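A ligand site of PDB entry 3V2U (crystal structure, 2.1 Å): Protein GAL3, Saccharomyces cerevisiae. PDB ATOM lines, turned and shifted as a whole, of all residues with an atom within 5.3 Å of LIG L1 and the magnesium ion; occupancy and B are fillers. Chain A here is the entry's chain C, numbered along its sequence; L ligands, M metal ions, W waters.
An oxygen (O5) of LIG L1 lies close to the backbone NH (N) of Ser 163.
The guanidinium group (NH1) of Arg 47 is in salt-bridge range of an oxygen (O3) of LIG L1, 2.7 Å away.
N of Gly 159 is in hydrogen-bond range of O4 of LIG L1, 2.7 Å away.
ND2 of Asn 89 lies within hydrogen-bond range of N4 of LIG L1 (2.9 Å).
The backbone NH (N) of Leu 162 is in hydrogen-bond range of an oxygen (O4) of LIG L1 (3.2 Å).
O3 of LIG L1 is in hydrogen-bond range of N of Gly 161 (2.9 Å).
The backbone NH (N) of Ala 460 is in hydrogen-bond range of an oxygen (O1) of LIG L1.
The side-chain amino group of Lys 258 lies within salt-bridge range of an oxygen (O7) of LIG L1.
N of Gly 160 sits at hydrogen-bond distance from O4 of LIG L1, 3.5 Å away.
The backbone NH (N) of Ala 460 lies within hydrogen-bond range of an oxygen (O5) of LG2 L2, 3.4 Å away.
The side-chain amino group (NZ) of Lys 258 sits at hydrogen-bond distance from an oxygen (O1) of LG2 L2 (3.4 Å).
OD2 of Asp 209 sits at hydrogen-bond distance from O2 of LG2 L2 (2.8 Å).
An oxygen (O1) of LG2 L2 is in hydrogen-bond range of an oxygen (O1) of LIG L1 (3.4 Å).
OG of Ser 163 lies close to OE1 of Glu 198 (2.6 Å).
O of Gly 159 lies within hydrogen-bond range of NH2 of Arg 47 (3.0 Å).
N of Arg 47 lies within hydrogen-bond range of O of Gly 160 (2.7 Å).
The guanidinium group (NE) of Arg 47 lies within salt-bridge range of the side-chain carboxylate (OD1) of Asp 209, 2.8 Å away.
The side-chain amide oxygen of Asn 89 sits at hydrogen-bond distance from the backbone NH of Asp 91.
The side-chain hydroxyl (OG) of Ser 154 lies within hydrogen-bond range of the backbone NH (N) of Ile 156 (3.0 Å).
Residues that only touch LIG L1: Phe 94 (3.3 Å), Tyr 120 (3.4 Å), Trp 117 (3.4 Å), Thr 158 (3.5 Å), Met 71 (3.6 Å), Ser 115 (3.8 Å), Pro 157 (3.8 Å), Asp 209 (3.8 Å), Phe 166 (3.9 Å), Gly 459 (3.96 Å) and Ser 154 (3.97 Å).
The nearest printed residue that does not touch the magnesium ion is Lys 258 (4.1 Å).
O5 of LIG L1 binds the magnesium ion, at 2.2 Å.
An oxygen (O8) of LIG L1 is bound to the magnesium ion (2.2 Å).
The magnesium ion is bound by OG of Ser 163 (2.2 Å).
An oxygen (O2) of LIG L1 binds the magnesium ion (2.2 Å).
The magnesium ion is bound by water W5 (2.3 Å).
Water W8 is bound to the magnesium ion, at 2.5 Å.
The magnesium ion has six donor atoms within binding distance.
Water W5 lies within hydrogen-bond range of OD2 of Asp 209 (2.5 Å), OG of Ser 164 (2.7 Å) and O2 of LG2 L2 (3.4 Å).
Water W1 lies within hydrogen-bond range of the side-chain hydroxyl of Ser 256 (2.6 Å), an oxygen (O7) of LIG L1 (2.8 Å) and the backbone NH of Lys 258 (3.0 Å).
Water W3 lies within hydrogen-bond range of an oxygen (O12) of LIG L1 and the side-chain hydroxyl (OG) of Ser 256.
Water W7 lies within hydrogen-bond range of O1 of LIG L1 (2.9 Å), N of Gly 461 (3.1 Å) and N of Ala 460 (3.4 Å).
Water W9 lies within hydrogen-bond range of OG of Ser 115 (3.0 Å), O12 of LIG L1 (3.0 Å) and OH of Tyr 120 (3.0 Å).
Water W6 bridges the side-chain hydroxyl (OG) of Ser 256 (2.8 Å) and the side-chain hydroxyl (OG1) of Thr 158 (3.1 Å).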
ATOM      1  N   ARG A  47      -8.290  -7.145   2.757  1.00  0.00           N
ATOM      2  CA  ARG A  47      -8.227  -7.503   1.349  1.00  0.00           C
ATOM      3  C   ARG A  47      -7.092  -8.468   1.032  1.00  0.00           C
ATOM      4  O   ARG A  47      -6.124  -8.566   1.782  1.00  0.00           O
ATOM      5  CB  ARG A  47      -8.056  -6.239   0.493  1.00  0.00           C
ATOM      6  CG  ARG A  47      -6.729  -5.535   0.717  1.00  0.00           C
ATOM      7  CD  ARG A  47      -5.621  -6.042  -0.206  1.00  0.00           C
ATOM      8  NE  ARG A  47      -4.334  -5.446   0.161  1.00  0.00           N
ATOM      9  CZ  ARG A  47      -3.460  -6.001   0.995  1.00  0.00           C
ATOM     10  NH1 ARG A  47      -2.329  -5.393   1.288  1.00  0.00           N
ATOM     11  NH2 ARG A  47      -3.721  -7.190   1.531  1.00  0.00           N
ATOM     12  N   MET A  71     -12.275  -4.606   9.947  1.00  0.00           N
ATOM     13  CA  MET A  71     -12.077  -3.795  11.132  1.00  0.00           C
ATOM     14  C   MET A  71     -13.414  -3.176  11.516  1.00  0.00           C
ATOM     15  O   MET A  71     -14.061  -2.537  10.691  1.00  0.00           O
ATOM     16  CB  MET A  71     -11.023  -2.718  10.883  1.00  0.00           C
ATOM     17  CG  MET A  71     -10.922  -1.685  11.997  1.00  0.00           C
ATOM     18  SD  MET A  71     -10.615  -2.340  13.645  1.00  0.00           S
ATOM     19  CE  MET A  71      -8.806  -2.361  13.678  1.00  0.00           C
ATOM     20  N   ASN A  89      -9.046  -1.551  22.270  1.00  0.00           N
ATOM     21  CA  ASN A  89      -8.920  -2.629  21.287  1.00  0.00           C
ATOM     22  C   ASN A  89      -9.364  -3.976  21.863  1.00  0.00           C
ATOM     23  O   ASN A  89      -9.144  -4.264  23.043  1.00  0.00           O
ATOM     24  CB  ASN A  89      -7.488  -2.737  20.784  1.00  0.00           C
ATOM     25  CG  ASN A  89      -7.395  -3.385  19.419  1.00  0.00           C
ATOM     26  OD1 ASN A  89      -7.673  -4.571  19.260  1.00  0.00           O
ATOM     27  ND2 ASN A  89      -7.000  -2.594  18.420  1.00  0.00           N
ATOM     28  N   ASP A  91      -8.081  -6.638  21.270  1.00  0.00           N
ATOM     29  CA  ASP A  91      -6.844  -7.354  21.555  1.00  0.00           C
ATOM     30  C   ASP A  91      -6.037  -6.574  22.586  1.00  0.00           C
ATOM     31  O   ASP A  91      -5.472  -5.518  22.285  1.00  0.00           O
ATOM     32  CB  ASP A  91      -6.028  -7.512  20.272  1.00  0.00           C
ATOM     33  CG  ASP A  91      -4.804  -8.368  20.464  1.00  0.00           C
ATOM     34  OD1 ASP A  91      -4.348  -8.509  21.622  1.00  0.00           O
ATOM     35  OD2 ASP A  91      -4.308  -8.911  19.460  1.00  0.00           O
ATOM     36  N   PHE A  94      -2.906  -4.251  22.363  1.00  0.00           N
ATOM     37  CA  PHE A  94      -2.999  -2.878  21.911  1.00  0.00           C
ATOM     38  C   PHE A  94      -3.662  -2.058  22.993  1.00  0.00           C
ATOM     39  O   PHE A  94      -4.887  -1.982  23.065  1.00  0.00           O
ATOM     40  CB  PHE A  94      -3.766  -2.797  20.599  1.00  0.00           C
ATOM     41  CG  PHE A  94      -3.140  -3.599  19.499  1.00  0.00           C
ATOM     42  CD1 PHE A  94      -1.886  -3.260  19.009  1.00  0.00           C
ATOM     43  CD2 PHE A  94      -3.779  -4.702  18.972  1.00  0.00           C
ATOM     44  CE1 PHE A  94      -1.284  -3.990  18.005  1.00  0.00           C
ATOM     45  CE2 PHE A  94      -3.199  -5.440  17.958  1.00  0.00           C
ATOM     46  CZ  PHE A  94      -1.944  -5.085  17.477  1.00  0.00           C
ATOM     47  N   SER A 115       6.231   2.926  16.285  1.00  0.00           N
ATOM     48  CA  SER A 115       5.124   2.079  15.885  1.00  0.00           C
ATOM     49  C   SER A 115       4.075   2.139  16.987  1.00  0.00           C
ATOM     50  O   SER A 115       4.369   1.855  18.132  1.00  0.00           O
ATOM     51  CB  SER A 115       5.610   0.640  15.714  1.00  0.00           C
ATOM     52  OG  SER A 115       4.538  -0.186  15.311  1.00  0.00           O
ATOM     53  N   GLU A 116       2.857   2.509  16.632  1.00  0.00           N
ATOM     54  CA  GLU A 116       1.783   2.667  17.597  1.00  0.00           C
ATOM     55  C   GLU A 116       0.435   2.489  16.903  1.00  0.00           C
ATOM     56  O   GLU A 116       0.124   3.171  15.922  1.00  0.00           O
ATOM     57  CB  GLU A 116       1.865   4.052  18.241  1.00  0.00           C
ATOM     58  CG  GLU A 116       0.560   4.559  18.844  1.00  0.00           C
ATOM     59  CD  GLU A 116       0.066   3.722  19.998  1.00  0.00           C
ATOM     60  OE1 GLU A 116       0.903   3.049  20.665  1.00  0.00           O
ATOM     61  OE2 GLU A 116      -1.159   3.713  20.243  1.00  0.00           O
ATOM     62  N   TRP A 117      -0.360   1.549  17.417  1.00  0.00           N
ATOM     63  CA  TRP A 117      -1.601   1.177  16.758  1.00  0.00           C
ATOM     64  C   TRP A 117      -2.567   2.345  16.627  1.00  0.00           C
ATOM     65  O   TRP A 117      -3.261   2.464  15.620  1.00  0.00           O
ATOM     66  CB  TRP A 117      -2.263  -0.026  17.462  1.00  0.00           C
ATOM     67  CG  TRP A 117      -2.947   0.309  18.757  1.00  0.00           C
ATOM     68  CD1 TRP A 117      -2.360   0.426  19.982  1.00  0.00           C
ATOM     69  CD2 TRP A 117      -4.352   0.528  18.957  1.00  0.00           C
ATOM     70  NE1 TRP A 117      -3.308   0.728  20.934  1.00  0.00           N
ATOM     71  CE2 TRP A 117      -4.546   0.793  20.335  1.00  0.00           C
ATOM     72  CE3 TRP A 117      -5.467   0.535  18.115  1.00  0.00           C
ATOM     73  CZ2 TRP A 117      -5.807   1.053  20.879  1.00  0.00           C
ATOM     74  CZ3 TRP A 117      -6.728   0.795  18.660  1.00  0.00           C
ATOM     75  CH2 TRP A 117      -6.877   1.055  20.035  1.00  0.00           C
ATOM     76  N   TYR A 120      -2.714   4.788  13.445  1.00  0.00           N
ATOM     77  CA  TYR A 120      -3.594   4.540  12.310  1.00  0.00           C
ATOM     78  C   TYR A 120      -4.962   5.210  12.498  1.00  0.00           C
ATOM     79  O   TYR A 120      -5.505   5.783  11.552  1.00  0.00           O
ATOM     80  CB  TYR A 120      -3.729   3.047  11.984  1.00  0.00           C
ATOM     81  CG  TYR A 120      -2.406   2.455  11.568  1.00  0.00           C
ATOM     82  CD1 TYR A 120      -1.930   2.617  10.271  1.00  0.00           C
ATOM     83  CD2 TYR A 120      -1.612   1.770  12.491  1.00  0.00           C
ATOM     84  CE1 TYR A 120      -0.704   2.100   9.899  1.00  0.00           C
ATOM     85  CE2 TYR A 120      -0.389   1.245  12.122  1.00  0.00           C
ATOM     86  CZ  TYR A 120       0.061   1.413  10.816  1.00  0.00           C
ATOM     87  OH  TYR A 120       1.282   0.895  10.435  1.00  0.00           O
ATOM     88  N   SER A 154     -10.696  -6.164  15.149  1.00  0.00           N
ATOM     89  CA  SER A 154     -10.364  -6.680  13.835  1.00  0.00           C
ATOM     90  C   SER A 154     -10.069  -8.163  13.910  1.00  0.00           C
ATOM     91  O   SER A 154      -9.452  -8.634  14.861  1.00  0.00           O
ATOM     92  CB  SER A 154      -9.121  -5.953  13.305  1.00  0.00           C
ATOM     93  OG  SER A 154      -8.790  -6.402  12.013  1.00  0.00           O
ATOM     94  N   ILE A 156      -8.917  -9.183  10.836  1.00  0.00           N
ATOM     95  CA  ILE A 156      -8.044  -9.156   9.657  1.00  0.00           C
ATOM     96  C   ILE A 156      -6.643  -9.595  10.056  1.00  0.00           C
ATOM     97  O   ILE A 156      -6.049  -9.012  10.962  1.00  0.00           O
ATOM     98  CB  ILE A 156      -7.937  -7.745   9.061  1.00  0.00           C
ATOM     99  CG1 ILE A 156      -9.317  -7.201   8.710  1.00  0.00           C
ATOM    100  CG2 ILE A 156      -7.000  -7.754   7.826  1.00  0.00           C
ATOM    101  CD1 ILE A 156      -9.298  -5.735   8.300  1.00  0.00           C
ATOM    102  N   PRO A 157      -6.106 -10.617   9.381  1.00  0.00           N
ATOM    103  CA  PRO A 157      -4.736 -11.029   9.710  1.00  0.00           C
ATOM    104  C   PRO A 157      -3.727 -10.048   9.127  1.00  0.00           C
ATOM    105  O   PRO A 157      -3.985  -9.436   8.079  1.00  0.00           O
ATOM    106  CB  PRO A 157      -4.629 -12.390   9.015  1.00  0.00           C
ATOM    107  CG  PRO A 157      -5.529 -12.261   7.835  1.00  0.00           C
ATOM    108  CD  PRO A 157      -6.690 -11.428   8.303  1.00  0.00           C
ATOM    109  N   THR A 158      -2.592  -9.888   9.789  1.00  0.00           N
ATOM    110  CA  THR A 158      -1.535  -9.010   9.294  1.00  0.00           C
ATOM    111  C   THR A 158      -1.171  -9.438   7.893  1.00  0.00           C
ATOM    112  O   THR A 158      -0.909 -10.627   7.640  1.00  0.00           O
ATOM    113  CB  THR A 158      -0.283  -9.058  10.155  1.00  0.00           C
ATOM    114  OG1 THR A 158      -0.645  -8.938  11.536  1.00  0.00           O
ATOM    115  CG2 THR A 158       0.670  -7.911   9.774  1.00  0.00           C
ATOM    116  N   GLY A 159      -1.201  -8.473   6.976  1.00  0.00           N
ATOM    117  CA  GLY A 159      -0.976  -8.771   5.574  1.00  0.00           C
ATOM    118  C   GLY A 159      -2.267  -8.724   4.785  1.00  0.00           C
ATOM    119  O   GLY A 159      -2.241  -8.804   3.567  1.00  0.00           O
ATOM    120  N   GLY A 160      -3.396  -8.590   5.490  1.00  0.00           N
ATOM    121  CA  GLY A 160      -4.691  -8.448   4.838  1.00  0.00           C
ATOM    122  C   GLY A 160      -5.165  -7.008   4.703  1.00  0.00           C
ATOM    123  O   GLY A 160      -6.359  -6.745   4.572  1.00  0.00           O
ATOM    124  N   GLY A 161      -4.228  -6.061   4.721  1.00  0.00           N
ATOM    125  CA  GLY A 161      -4.571  -4.670   4.528  1.00  0.00           C
ATOM    126  C   GLY A 161      -5.270  -4.069   5.739  1.00  0.00           C
ATOM    127  O   GLY A 161      -6.043  -3.124   5.620  1.00  0.00           O
ATOM    128  N   LEU A 162      -4.997  -4.632   6.910  1.00  0.00           N
ATOM    129  CA  LEU A 162      -5.584  -4.170   8.154  1.00  0.00           C
ATOM    130  C   LEU A 162      -5.336  -2.673   8.372  1.00  0.00           C
ATOM    131  O   LEU A 162      -6.246  -1.943   8.755  1.00  0.00           O
ATOM    132  CB  LEU A 162      -5.020  -4.958   9.336  1.00  0.00           C
ATOM    133  CG  LEU A 162      -5.642  -4.647  10.706  1.00  0.00           C
ATOM    134  CD1 LEU A 162      -5.484  -5.829  11.651  1.00  0.00           C
ATOM    135  CD2 LEU A 162      -5.052  -3.368  11.310  1.00  0.00           C
ATOM    136  N   SER A 163      -4.106  -2.225   8.138  1.00  0.00           N
ATOM    137  CA  SER A 163      -3.774  -0.834   8.446  1.00  0.00           C
ATOM    138  C   SER A 163      -4.653   0.134   7.659  1.00  0.00           C
ATOM    139  O   SER A 163      -5.117   1.139   8.196  1.00  0.00           O
ATOM    140  CB  SER A 163      -2.278  -0.545   8.249  1.00  0.00           C
ATOM    141  OG  SER A 163      -1.943  -0.411   6.877  1.00  0.00           O
ATOM    142  N   SER A 164      -4.920  -0.181   6.398  1.00  0.00           N
ATOM    143  CA  SER A 164      -5.789   0.633   5.554  1.00  0.00           C
ATOM    144  C   SER A 164      -7.281   0.516   5.915  1.00  0.00           C
ATOM    145  O   SER A 164      -8.006   1.523   5.873  1.00  0.00           O
ATOM    146  CB  SER A 164      -5.569   0.303   4.077  1.00  0.00           C
ATOM    147  OG  SER A 164      -4.196   0.421   3.753  1.00  0.00           O
ATOM    148  N   PHE A 166      -8.423  -0.047   8.834  1.00  0.00           N
ATOM    149  CA  PHE A 166      -8.484   0.728  10.068  1.00  0.00           C
ATOM    150  C   PHE A 166      -8.543   2.225   9.771  1.00  0.00           C
ATOM    151  O   PHE A 166      -9.402   2.935  10.281  1.00  0.00           O
ATOM    152  CB  PHE A 166      -7.300   0.391  10.973  1.00  0.00           C
ATOM    153  CG  PHE A 166      -7.417   0.948  12.372  1.00  0.00           C
ATOM    154  CD1 PHE A 166      -8.631   1.369  12.877  1.00  0.00           C
ATOM    155  CD2 PHE A 166      -6.290   1.028  13.188  1.00  0.00           C
ATOM    156  CE1 PHE A 166      -8.733   1.864  14.173  1.00  0.00           C
ATOM    157  CE2 PHE A 166      -6.387   1.510  14.484  1.00  0.00           C
ATOM    158  CZ  PHE A 166      -7.603   1.938  14.977  1.00  0.00           C
ATOM    159  N   GLU A 198      -1.682   7.011   5.566  1.00  0.00           N
ATOM    160  CA  GLU A 198      -0.584   6.298   6.223  1.00  0.00           C
ATOM    161  C   GLU A 198       0.749   6.986   6.100  1.00  0.00           C
ATOM    162  O   GLU A 198       1.659   6.738   6.905  1.00  0.00           O
ATOM    163  CB  GLU A 198      -0.469   4.848   5.722  1.00  0.00           C
ATOM    164  CG  GLU A 198      -1.349   3.882   6.449  1.00  0.00           C
ATOM    165  CD  GLU A 198      -1.201   2.458   5.958  1.00  0.00           C
ATOM    166  OE1 GLU A 198      -2.243   1.861   5.631  1.00  0.00           O
ATOM    167  OE2 GLU A 198      -0.063   1.928   5.906  1.00  0.00           O
ATOM    168  N   ASP A 209      -5.145  -0.618  -1.186  1.00  0.00           N
ATOM    169  CA  ASP A 209      -5.858  -1.174  -0.040  1.00  0.00           C
ATOM    170  C   ASP A 209      -7.062  -0.318   0.366  1.00  0.00           C
ATOM    171  O   ASP A 209      -8.131  -0.858   0.652  1.00  0.00           O
ATOM    172  CB  ASP A 209      -4.920  -1.357   1.152  1.00  0.00           C
ATOM    173  CG  ASP A 209      -3.707  -2.210   0.813  1.00  0.00           C
ATOM    174  OD1 ASP A 209      -3.687  -2.806  -0.280  1.00  0.00           O
ATOM    175  OD2 ASP A 209      -2.768  -2.289   1.635  1.00  0.00           O
ATOM    176  N   SER A 256       5.029  -9.282  13.086  1.00  0.00           N
ATOM    177  CA  SER A 256       4.711  -8.041  12.383  1.00  0.00           C
ATOM    178  C   SER A 256       5.666  -6.911  12.757  1.00  0.00           C
ATOM    179  O   SER A 256       5.790  -6.549  13.929  1.00  0.00           O
ATOM    180  CB  SER A 256       3.274  -7.617  12.714  1.00  0.00           C
ATOM    181  OG  SER A 256       2.977  -6.318  12.213  1.00  0.00           O
ATOM    182  N   LYS A 258       6.437  -4.030   9.989  1.00  0.00           N
ATOM    183  CA  LYS A 258       6.562  -3.237   8.773  1.00  0.00           C
ATOM    184  C   LYS A 258       7.112  -1.848   9.068  1.00  0.00           C
ATOM    185  O   LYS A 258       7.992  -1.372   8.350  1.00  0.00           O
ATOM    186  CB  LYS A 258       5.222  -3.133   8.050  1.00  0.00           C
ATOM    187  CG  LYS A 258       5.303  -2.535   6.641  1.00  0.00           C
ATOM    188  CD  LYS A 258       4.157  -1.552   6.409  1.00  0.00           C
ATOM    189  CE  LYS A 258       3.362  -1.889   5.169  1.00  0.00           C
ATOM    190  NZ  LYS A 258       2.775  -3.251   5.274  1.00  0.00           N
ATOM    191  N   GLY A 459      -0.176  -8.628  -0.257  1.00  0.00           N
ATOM    192  CA  GLY A 459       0.175  -7.515   0.613  1.00  0.00           C
ATOM    193  C   GLY A 459       1.641  -7.147   0.441  1.00  0.00           C
ATOM    194  O   GLY A 459       2.252  -7.482  -0.570  1.00  0.00           O
ATOM    195  N   ALA A 460       2.217  -6.473   1.434  1.00  0.00           N
ATOM    196  CA  ALA A 460       3.605  -5.999   1.311  1.00  0.00           C
ATOM    197  C   ALA A 460       4.640  -7.125   1.306  1.00  0.00           C
ATOM    198  O   ALA A 460       5.637  -7.066   0.594  1.00  0.00           O
ATOM    199  CB  ALA A 460       3.910  -5.004   2.426  1.00  0.00           C
ATOM    200  N   GLY A 461       4.422  -8.157   2.105  1.00  0.00           N
ATOM    201  CA  GLY A 461       5.396  -9.239   2.177  1.00  0.00           C
ATOM    202  C   GLY A 461       6.314  -9.083   3.368  1.00  0.00           C
ATOM    203  O   GLY A 461       5.943  -8.479   4.377  1.00  0.00           O
HETATM  204  P1  LIG L   1      -0.292  -5.063   4.559  1.00  0.00           P
HETATM  205  O1  LIG L   1       0.989  -5.648   4.048  1.00  0.00           O
HETATM  206  O2  LIG L   1      -0.282  -3.602   4.264  1.00  0.00           O
HETATM  207  O3  LIG L   1      -1.472  -5.743   3.797  1.00  0.00           O
HETATM  208  P2  LIG L   1      -1.371  -4.890   7.114  1.00  0.00           P
HETATM  209  O4  LIG L   1      -2.248  -6.047   7.534  1.00  0.00           O
HETATM  210  O5  LIG L   1      -2.297  -3.704   6.739  1.00  0.00           O
HETATM  211  O6  LIG L   1      -0.359  -5.385   6.008  1.00  0.00           O
HETATM  212  P3  LIG L   1       0.575  -3.317   8.369  1.00  0.00           P
HETATM  213  O7  LIG L   1       1.941  -3.929   8.313  1.00  0.00           O
HETATM  214  O8  LIG L   1       0.410  -2.428   7.217  1.00  0.00           O
HETATM  215  O9  LIG L   1      -0.536  -4.449   8.391  1.00  0.00           O
HETATM  216  O10 LIG L   1       0.402  -2.486   9.744  1.00  0.00           O
HETATM  217  C1  LIG L   1       0.455  -3.131  10.997  1.00  0.00           C
HETATM  218  C2  LIG L   1       0.119  -2.282  12.123  1.00  0.00           C
HETATM  219  O11 LIG L   1      -1.258  -2.271  12.290  1.00  0.00           O
HETATM  220  C3  LIG L   1       0.648  -2.836  13.420  1.00  0.00           C
HETATM  221  O12 LIG L   1       1.957  -2.417  13.608  1.00  0.00           O
HETATM  222  C4  LIG L   1      -0.218  -2.255  14.393  1.00  0.00           C
HETATM  223  O13 LIG L   1       0.162  -0.944  14.689  1.00  0.00           O
HETATM  224  C5  LIG L   1      -1.526  -2.207  13.697  1.00  0.00           C
HETATM  225  N1  LIG L   1      -2.416  -3.278  14.095  1.00  0.00           N
HETATM  226  C6  LIG L   1      -2.189  -4.587  13.960  1.00  0.00           C
HETATM  227  N2  LIG L   1      -3.246  -5.261  14.448  1.00  0.00           N
HETATM  228  C7  LIG L   1      -4.150  -4.356  14.896  1.00  0.00           C
HETATM  229  C8  LIG L   1      -5.409  -4.442  15.490  1.00  0.00           C
HETATM  230  N3  LIG L   1      -5.995  -5.754  15.739  1.00  0.00           N
HETATM  231  N4  LIG L   1      -6.090  -3.326  15.815  1.00  0.00           N
HETATM  232  C9  LIG L   1      -5.550  -2.107  15.578  1.00  0.00           C
HETATM  233  N5  LIG L   1      -4.329  -1.989  15.025  1.00  0.00           N
HETATM  234  C10 LIG L   1      -3.627  -3.091  14.672  1.00  0.00           C
HETATM  235  C1  LG2 L   2       1.369  -2.312   1.030  1.00  0.00           C
HETATM  236  C2  LG2 L   2       0.491  -1.123   0.649  1.00  0.00           C
HETATM  237  C3  LG2 L   2      -0.178  -1.224  -0.661  1.00  0.00           C
HETATM  238  C4  LG2 L   2       0.570  -1.938  -1.616  1.00  0.00           C
HETATM  239  C5  LG2 L   2       0.863  -3.336  -1.162  1.00  0.00           C
HETATM  240  C6  LG2 L   2       1.788  -4.031  -2.087  1.00  0.00           C
HETATM  241  O1  LG2 L   2       1.134  -2.731   2.329  1.00  0.00           O
HETATM  242  O2  LG2 L   2      -0.419  -0.748   1.693  1.00  0.00           O
HETATM  243  O3  LG2 L   2      -0.353   0.172  -1.127  1.00  0.00           O
HETATM  244  O4  LG2 L   2       1.819  -1.272  -1.885  1.00  0.00           O
HETATM  245  O5  LG2 L   2       1.466  -3.410   0.190  1.00  0.00           O
HETATM  246  O6  LG2 L   2       1.310  -4.516  -3.277  1.00  0.00           O
HETATM  247 MG    MG M   1      -1.168  -2.130   5.715  1.00  0.00          MG
HETATM  248  O   HOH W   1       3.687  -5.207  10.018  1.00  0.00           O
HETATM  249  O   HOH W   2      -8.776  -6.050  17.247  1.00  0.00           O
HETATM  250  O   HOH W   3       2.990  -4.654  15.003  1.00  0.00           O
HETATM  251  O   HOH W   4       1.319   0.249   7.790  1.00  0.00           O
HETATM  252  O   HOH W   5      -2.685  -1.762   4.028  1.00  0.00           O
HETATM  253  O   HOH W   6       0.184  -6.199  12.636  1.00  0.00           O
HETATM  254  O   HOH W   7       2.291  -8.216   4.320  1.00  0.00           O
HETATM  255  O   HOH W   8       0.184  -0.576   4.378  1.00  0.00           O
HETATM  256  O   HOH W   9       3.116   0.184  12.728  1.00  0.00           O
HETATM  257  O   HOH W  10       2.171  -0.871  16.658  1.00  0.00           O
